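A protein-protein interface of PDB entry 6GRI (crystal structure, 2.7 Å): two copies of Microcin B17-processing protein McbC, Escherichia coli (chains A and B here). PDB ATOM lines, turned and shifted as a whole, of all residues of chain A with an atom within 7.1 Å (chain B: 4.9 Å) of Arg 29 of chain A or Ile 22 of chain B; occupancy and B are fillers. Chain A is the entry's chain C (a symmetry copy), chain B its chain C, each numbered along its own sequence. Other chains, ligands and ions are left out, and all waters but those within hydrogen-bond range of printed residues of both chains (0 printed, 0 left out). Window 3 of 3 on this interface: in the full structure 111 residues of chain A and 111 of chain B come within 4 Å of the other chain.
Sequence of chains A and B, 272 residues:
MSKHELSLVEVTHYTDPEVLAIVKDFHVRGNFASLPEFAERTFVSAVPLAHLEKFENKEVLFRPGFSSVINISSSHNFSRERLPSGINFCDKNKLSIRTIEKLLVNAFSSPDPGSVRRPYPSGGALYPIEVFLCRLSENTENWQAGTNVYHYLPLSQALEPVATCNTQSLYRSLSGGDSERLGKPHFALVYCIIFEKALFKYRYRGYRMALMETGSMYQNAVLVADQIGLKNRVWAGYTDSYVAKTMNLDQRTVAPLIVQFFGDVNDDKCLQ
CE1 of Phe 26 of chain A touches CA of Val 23 of chain B, 3.9 Å away. Phe 26 of chain A touches Phe 26 of chain B (CD2 to CD2, 3.4 Å). CG2 of Ile 22 of chain B touches NE of Arg 29 of chain A, at 3.6 Å. Tyr 204 of chain B touches Arg 29 of chain A (CB to O, 3.4 Å). Gly 30 of chain A touches Tyr 204 of chain B (N to CB, 3.7 Å).
Arg 29 of chain A touches two residues of chain B. Ile 22 of chain B touches just one residue of chain A: Arg 29. Of the printed residues of chain A, Val 23 of chain B touches Phe 26. Printed residues of chain B within 4 Å of Gly 30 of chain A: Tyr 204 (3.7 Å). Printed residues of chain A within 4 Å of Phe 26 of chain B: Phe 26 (3.4 Å). Printed residues of chain B within 4 Å of Phe 26 of chain A: Val 23 and Phe 26. Printed residues of chain A within 4 Å of Tyr 204 of chain B: Arg 29 (3.4 Å) and Gly 30 (3.7 Å). Phe 32 of chain A touches none of the printed residues of chain B. The nearest printed residue of chain B that does not touch Arg 29 of chain A is Glu 18 of chain B (6.2 Å). The nearest residue of chain A that does not touch Ile 22 of chain B is Phe 26 of chain A (4.1 Å).
Hydrophobic or aromatic side chains of chain A within 4 Å of the printed part of chain B: Phe 26. Printed residues of chain B that touch a printed residue of chain A: Ile 22, Val 23, Phe 26 and Tyr 204.
Phe 26 of chain A touches its own counterpart, Phe 26 of chain B. 4 positions are printed for both chains.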
ATOM      1  N   ILE A  22      -7.351  17.409   4.210  1.00  0.00           N
ATOM      2  CA  ILE A  22      -5.881  17.401   4.113  1.00  0.00           C
ATOM      3  C   ILE A  22      -5.345  17.968   2.774  1.00  0.00           C
ATOM      4  O   ILE A  22      -4.337  18.678   2.758  1.00  0.00           O
ATOM      5  CB  ILE A  22      -5.344  15.971   4.416  1.00  0.00           C
ATOM      6  CG1 ILE A  22      -5.375  15.738   5.928  1.00  0.00           C
ATOM      7  CG2 ILE A  22      -3.931  15.758   3.896  1.00  0.00           C
ATOM      8  CD1 ILE A  22      -5.331  14.283   6.326  1.00  0.00           C
ATOM      9  N   LYS A  24      -7.079  20.168   0.826  1.00  0.00           N
ATOM     10  CA  LYS A  24      -7.409  21.595   0.876  1.00  0.00           C
ATOM     11  C   LYS A  24      -6.441  22.386   1.763  1.00  0.00           C
ATOM     12  O   LYS A  24      -5.963  23.432   1.344  1.00  0.00           O
ATOM     13  CB  LYS A  24      -8.827  21.811   1.397  1.00  0.00           C
ATOM     14  CG  LYS A  24      -9.960  21.496   0.432  1.00  0.00           C
ATOM     15  CD  LYS A  24     -11.271  21.543   1.201  1.00  0.00           C
ATOM     16  CE  LYS A  24     -12.460  21.754   0.289  1.00  0.00           C
ATOM     17  NZ  LYS A  24     -13.687  22.083   1.069  1.00  0.00           N
ATOM     18  N   ASP A  25      -6.169  21.892   2.979  1.00  0.00           N
ATOM     19  CA  ASP A  25      -5.146  22.478   3.893  1.00  0.00           C
ATOM     20  C   ASP A  25      -3.798  22.685   3.228  1.00  0.00           C
ATOM     21  O   ASP A  25      -3.095  23.640   3.555  1.00  0.00           O
ATOM     22  CB  ASP A  25      -4.860  21.587   5.093  1.00  0.00           C
ATOM     23  CG  ASP A  25      -6.030  21.445   6.032  1.00  0.00           C
ATOM     24  OD1 ASP A  25      -7.077  22.106   5.837  1.00  0.00           O
ATOM     25  OD2 ASP A  25      -5.896  20.642   6.989  1.00  0.00           O
ATOM     26  N   PHE A  26      -3.426  21.758   2.339  1.00  0.00           N
ATOM     27  CA  PHE A  26      -2.160  21.830   1.621  1.00  0.00           C
ATOM     28  C   PHE A  26      -2.274  22.837   0.516  1.00  0.00           C
ATOM     29  O   PHE A  26      -1.479  23.749   0.426  1.00  0.00           O
ATOM     30  CB  PHE A  26      -1.749  20.464   1.039  1.00  0.00           C
ATOM     31  CG  PHE A  26      -0.502  20.526   0.220  1.00  0.00           C
ATOM     32  CD1 PHE A  26       0.726  20.678   0.831  1.00  0.00           C
ATOM     33  CD2 PHE A  26      -0.556  20.490  -1.162  1.00  0.00           C
ATOM     34  CE1 PHE A  26       1.891  20.770   0.085  1.00  0.00           C
ATOM     35  CE2 PHE A  26       0.607  20.580  -1.920  1.00  0.00           C
ATOM     36  CZ  PHE A  26       1.835  20.724  -1.289  1.00  0.00           C
ATOM     37  N   HIS A  27      -3.272  22.649  -0.330  1.00  0.00           N
ATOM     38  CA  HIS A  27      -3.559  23.557  -1.430  1.00  0.00           C
ATOM     39  C   HIS A  27      -3.449  25.039  -1.071  1.00  0.00           C
ATOM     40  O   HIS A  27      -2.834  25.812  -1.787  1.00  0.00           O
ATOM     41  CB  HIS A  27      -4.972  23.294  -1.957  1.00  0.00           C
ATOM     42  CG  HIS A  27      -5.288  24.068  -3.187  1.00  0.00           C
ATOM     43  ND1 HIS A  27      -4.978  23.607  -4.443  1.00  0.00           N
ATOM     44  CD2 HIS A  27      -5.833  25.295  -3.353  1.00  0.00           C
ATOM     45  CE1 HIS A  27      -5.334  24.512  -5.335  1.00  0.00           C
ATOM     46  NE2 HIS A  27      -5.856  25.547  -4.701  1.00  0.00           N
ATOM     47  N   VAL A  28      -4.051  25.412   0.047  1.00  0.00           N
ATOM     48  CA  VAL A  28      -4.131  26.807   0.499  1.00  0.00           C
ATOM     49  C   VAL A  28      -2.771  27.438   0.884  1.00  0.00           C
ATOM     50  O   VAL A  28      -2.637  28.677   0.930  1.00  0.00           O
ATOM     51  CB  VAL A  28      -5.196  26.919   1.630  1.00  0.00           C
ATOM     52  CG1 VAL A  28      -5.176  28.270   2.311  1.00  0.00           C
ATOM     53  CG2 VAL A  28      -6.586  26.676   1.045  1.00  0.00           C
ATOM     54  N   ARG A  29      -1.762  26.601   1.121  1.00  0.00           N
ATOM     55  CA  ARG A  29      -0.404  27.077   1.421  1.00  0.00           C
ATOM     56  C   ARG A  29       0.236  27.770   0.220  1.00  0.00           C
ATOM     57  O   ARG A  29       1.136  28.598   0.376  1.00  0.00           O
ATOM     58  CB  ARG A  29       0.496  25.922   1.858  1.00  0.00           C
ATOM     59  CG  ARG A  29       0.057  25.219   3.130  1.00  0.00           C
ATOM     60  CD  ARG A  29       0.965  24.034   3.382  1.00  0.00           C
ATOM     61  NE  ARG A  29       0.563  23.274   4.562  1.00  0.00           N
ATOM     62  CZ  ARG A  29       0.756  23.659   5.815  1.00  0.00           C
ATOM     63  NH1 ARG A  29       1.331  24.817   6.103  1.00  0.00           N
ATOM     64  NH2 ARG A  29       0.355  22.878   6.800  1.00  0.00           N
ATOM     65  N   GLY A  30      -0.228  27.415  -0.973  1.00  0.00           N
ATOM     66  CA  GLY A  30       0.280  27.987  -2.195  1.00  0.00           C
ATOM     67  C   GLY A  30      -0.599  29.062  -2.774  1.00  0.00           C
ATOM     68  O   GLY A  30      -0.363  29.480  -3.902  1.00  0.00           O
ATOM     69  N   ASN A  31      -1.605  29.519  -2.027  1.00  0.00           N
ATOM     70  CA  ASN A  31      -2.431  30.635  -2.486  1.00  0.00           C
ATOM     71  C   ASN A  31      -1.668  31.901  -2.216  1.00  0.00           C
ATOM     72  O   ASN A  31      -0.976  31.999  -1.215  1.00  0.00           O
ATOM     73  CB  ASN A  31      -3.788  30.692  -1.772  1.00  0.00           C
ATOM     74  CG  ASN A  31      -4.784  29.687  -2.309  1.00  0.00           C
ATOM     75  OD1 ASN A  31      -4.643  29.183  -3.414  1.00  0.00           O
ATOM     76  ND2 ASN A  31      -5.806  29.403  -1.524  1.00  0.00           N
ATOM     77  N   PHE A  32      -1.825  32.868  -3.108  1.00  0.00           N
ATOM     78  CA  PHE A  32      -1.140  34.148  -3.041  1.00  0.00           C
ATOM     79  C   PHE A  32      -2.107  35.259  -2.652  1.00  0.00           C
ATOM     80  O   PHE A  32      -3.307  35.195  -2.941  1.00  0.00           O
ATOM     81  CB  PHE A  32      -0.527  34.467  -4.416  1.00  0.00           C
ATOM     82  CG  PHE A  32       0.825  33.850  -4.664  1.00  0.00           C
ATOM     83  CD1 PHE A  32       1.361  32.840  -3.841  1.00  0.00           C
ATOM     84  CD2 PHE A  32       1.563  34.273  -5.749  1.00  0.00           C
ATOM     85  CE1 PHE A  32       2.609  32.299  -4.091  1.00  0.00           C
ATOM     86  CE2 PHE A  32       2.810  33.725  -6.013  1.00  0.00           C
ATOM     87  CZ  PHE A  32       3.336  32.743  -5.184  1.00  0.00           C
ATOM     88  N   GLU B  18      11.275  24.062   6.224  1.00  0.00           N
ATOM     89  CA  GLU B  18       9.876  23.873   6.644  1.00  0.00           C
ATOM     90  C   GLU B  18       9.020  23.613   5.412  1.00  0.00           C
ATOM     91  O   GLU B  18       8.212  22.687   5.407  1.00  0.00           O
ATOM     92  CB  GLU B  18       9.344  25.092   7.402  1.00  0.00           C
ATOM     93  CG  GLU B  18       7.872  25.045   7.848  1.00  0.00           C
ATOM     94  CD  GLU B  18       7.632  24.429   9.225  1.00  0.00           C
ATOM     95  OE1 GLU B  18       8.586  23.967   9.899  1.00  0.00           O
ATOM     96  OE2 GLU B  18       6.457  24.407   9.643  1.00  0.00           O
ATOM     97  N   VAL B  19       9.207  24.403   4.357  1.00  0.00           N
ATOM     98  CA  VAL B  19       8.417  24.197   3.144  1.00  0.00           C
ATOM     99  C   VAL B  19       8.709  22.827   2.539  1.00  0.00           C
ATOM    100  O   VAL B  19       7.783  22.125   2.103  1.00  0.00           O
ATOM    101  CB  VAL B  19       8.636  25.284   2.082  1.00  0.00           C
ATOM    102  CG1 VAL B  19       7.851  24.959   0.820  1.00  0.00           C
ATOM    103  CG2 VAL B  19       8.223  26.647   2.611  1.00  0.00           C
ATOM    104  N   LEU B  20       9.988  22.444   2.515  1.00  0.00           N
ATOM    105  CA  LEU B  20      10.390  21.220   1.824  1.00  0.00           C
ATOM    106  C   LEU B  20       9.785  20.008   2.507  1.00  0.00           C
ATOM    107  O   LEU B  20       9.210  19.147   1.852  1.00  0.00           O
ATOM    108  CB  LEU B  20      11.904  21.098   1.800  1.00  0.00           C
ATOM    109  CG  LEU B  20      12.503  19.928   1.030  1.00  0.00           C
ATOM    110  CD1 LEU B  20      12.251  20.067  -0.471  1.00  0.00           C
ATOM    111  CD2 LEU B  20      13.987  19.836   1.336  1.00  0.00           C
ATOM    112  N   ALA B  21       9.917  19.957   3.828  1.00  0.00           N
ATOM    113  CA  ALA B  21       9.344  18.880   4.634  1.00  0.00           C
ATOM    114  C   ALA B  21       7.828  18.720   4.439  1.00  0.00           C
ATOM    115  O   ALA B  21       7.347  17.610   4.260  1.00  0.00           O
ATOM    116  CB  ALA B  21       9.646  19.124   6.101  1.00  0.00           C
ATOM    117  N   ILE B  22       7.098  19.835   4.483  1.00  0.00           N
ATOM    118  CA  ILE B  22       5.630  19.854   4.355  1.00  0.00           C
ATOM    119  C   ILE B  22       5.125  19.415   2.957  1.00  0.00           C
ATOM    120  O   ILE B  22       4.117  18.711   2.853  1.00  0.00           O
ATOM    121  CB  ILE B  22       5.085  21.250   4.777  1.00  0.00           C
ATOM    122  CG1 ILE B  22       5.082  21.341   6.305  1.00  0.00           C
ATOM    123  CG2 ILE B  22       3.684  21.512   4.248  1.00  0.00           C
ATOM    124  CD1 ILE B  22       5.028  22.752   6.836  1.00  0.00           C
ATOM    125  N   VAL B  23       5.839  19.811   1.902  1.00  0.00           N
ATOM    126  CA  VAL B  23       5.522  19.395   0.530  1.00  0.00           C
ATOM    127  C   VAL B  23       5.777  17.902   0.334  1.00  0.00           C
ATOM    128  O   VAL B  23       4.968  17.221  -0.294  1.00  0.00           O
ATOM    129  CB  VAL B  23       6.338  20.197  -0.506  1.00  0.00           C
ATOM    130  CG1 VAL B  23       6.113  19.681  -1.917  1.00  0.00           C
ATOM    131  CG2 VAL B  23       5.984  21.678  -0.446  1.00  0.00           C
ATOM    132  N   LYS B  24       6.903  17.404   0.851  1.00  0.00           N
ATOM    133  CA  LYS B  24       7.233  15.978   0.775  1.00  0.00           C
ATOM    134  C   LYS B  24       6.247  15.109   1.563  1.00  0.00           C
ATOM    135  O   LYS B  24       5.779  14.108   1.037  1.00  0.00           O
ATOM    136  CB  LYS B  24       8.639  15.713   1.305  1.00  0.00           C
ATOM    137  CG  LYS B  24       9.794  16.116   0.398  1.00  0.00           C
ATOM    138  CD  LYS B  24      11.087  15.996   1.188  1.00  0.00           C
ATOM    139  CE  LYS B  24      12.296  15.870   0.287  1.00  0.00           C
ATOM    140  NZ  LYS B  24      13.506  15.468   1.060  1.00  0.00           N
ATOM    141  N   ASP B  25       5.948  15.488   2.813  1.00  0.00           N
ATOM    142  CA  ASP B  25       4.905  14.820   3.646  1.00  0.00           C
ATOM    143  C   ASP B  25       3.572  14.677   2.935  1.00  0.00           C
ATOM    144  O   ASP B  25       2.863  13.697   3.156  1.00  0.00           O
ATOM    145  CB  ASP B  25       4.592  15.596   4.917  1.00  0.00           C
ATOM    146  CG  ASP B  25       5.741  15.648   5.891  1.00  0.00           C
ATOM    147  OD1 ASP B  25       6.792  15.008   5.658  1.00  0.00           O
ATOM    148  OD2 ASP B  25       5.585  16.359   6.915  1.00  0.00           O
ATOM    149  N   PHE B  26       3.219  15.684   2.129  1.00  0.00           N
ATOM    150  CA  PHE B  26       1.970  15.681   1.379  1.00  0.00           C
ATOM    151  C   PHE B  26       2.109  14.780   0.188  1.00  0.00           C
ATOM    152  O   PHE B  26       1.317  13.882  -0.005  1.00  0.00           O
ATOM    153  CB  PHE B  26       1.570  17.095   0.918  1.00  0.00           C
ATOM    154  CG  PHE B  26       0.341  17.111   0.069  1.00  0.00           C
ATOM    155  CD1 PHE B  26      -0.900  16.904   0.637  1.00  0.00           C
ATOM    156  CD2 PHE B  26       0.426  17.275  -1.302  1.00  0.00           C
ATOM    157  CE1 PHE B  26      -2.048  16.883  -0.140  1.00  0.00           C
ATOM    158  CE2 PHE B  26      -0.721  17.258  -2.090  1.00  0.00           C
ATOM    159  CZ  PHE B  26      -1.962  17.057  -1.502  1.00  0.00           C
ATOM    160  N   TYR B 204       5.448  27.092  -1.671  1.00  0.00           N
ATOM    161  CA  TYR B 204       4.383  26.092  -1.881  1.00  0.00           C
ATOM    162  C   TYR B 204       3.748  26.122  -3.269  1.00  0.00           C
ATOM    163  O   TYR B 204       3.487  25.084  -3.847  1.00  0.00           O
ATOM    164  CB  TYR B 204       3.297  26.257  -0.816  1.00  0.00           C
ATOM    165  CG  TYR B 204       3.785  25.931   0.572  1.00  0.00           C
ATOM    166  CD1 TYR B 204       4.055  24.617   0.934  1.00  0.00           C
ATOM    167  CD2 TYR B 204       4.005  26.935   1.513  1.00  0.00           C
ATOM    168  CE1 TYR B 204       4.502  24.306   2.207  1.00  0.00           C
ATOM    169  CE2 TYR B 204       4.460  26.638   2.791  1.00  0.00           C
ATOM    170  CZ  TYR B 204       4.710  25.326   3.124  1.00  0.00           C
ATOM    171  OH  TYR B 204       5.174  25.012   4.369  1.00  0.00           O
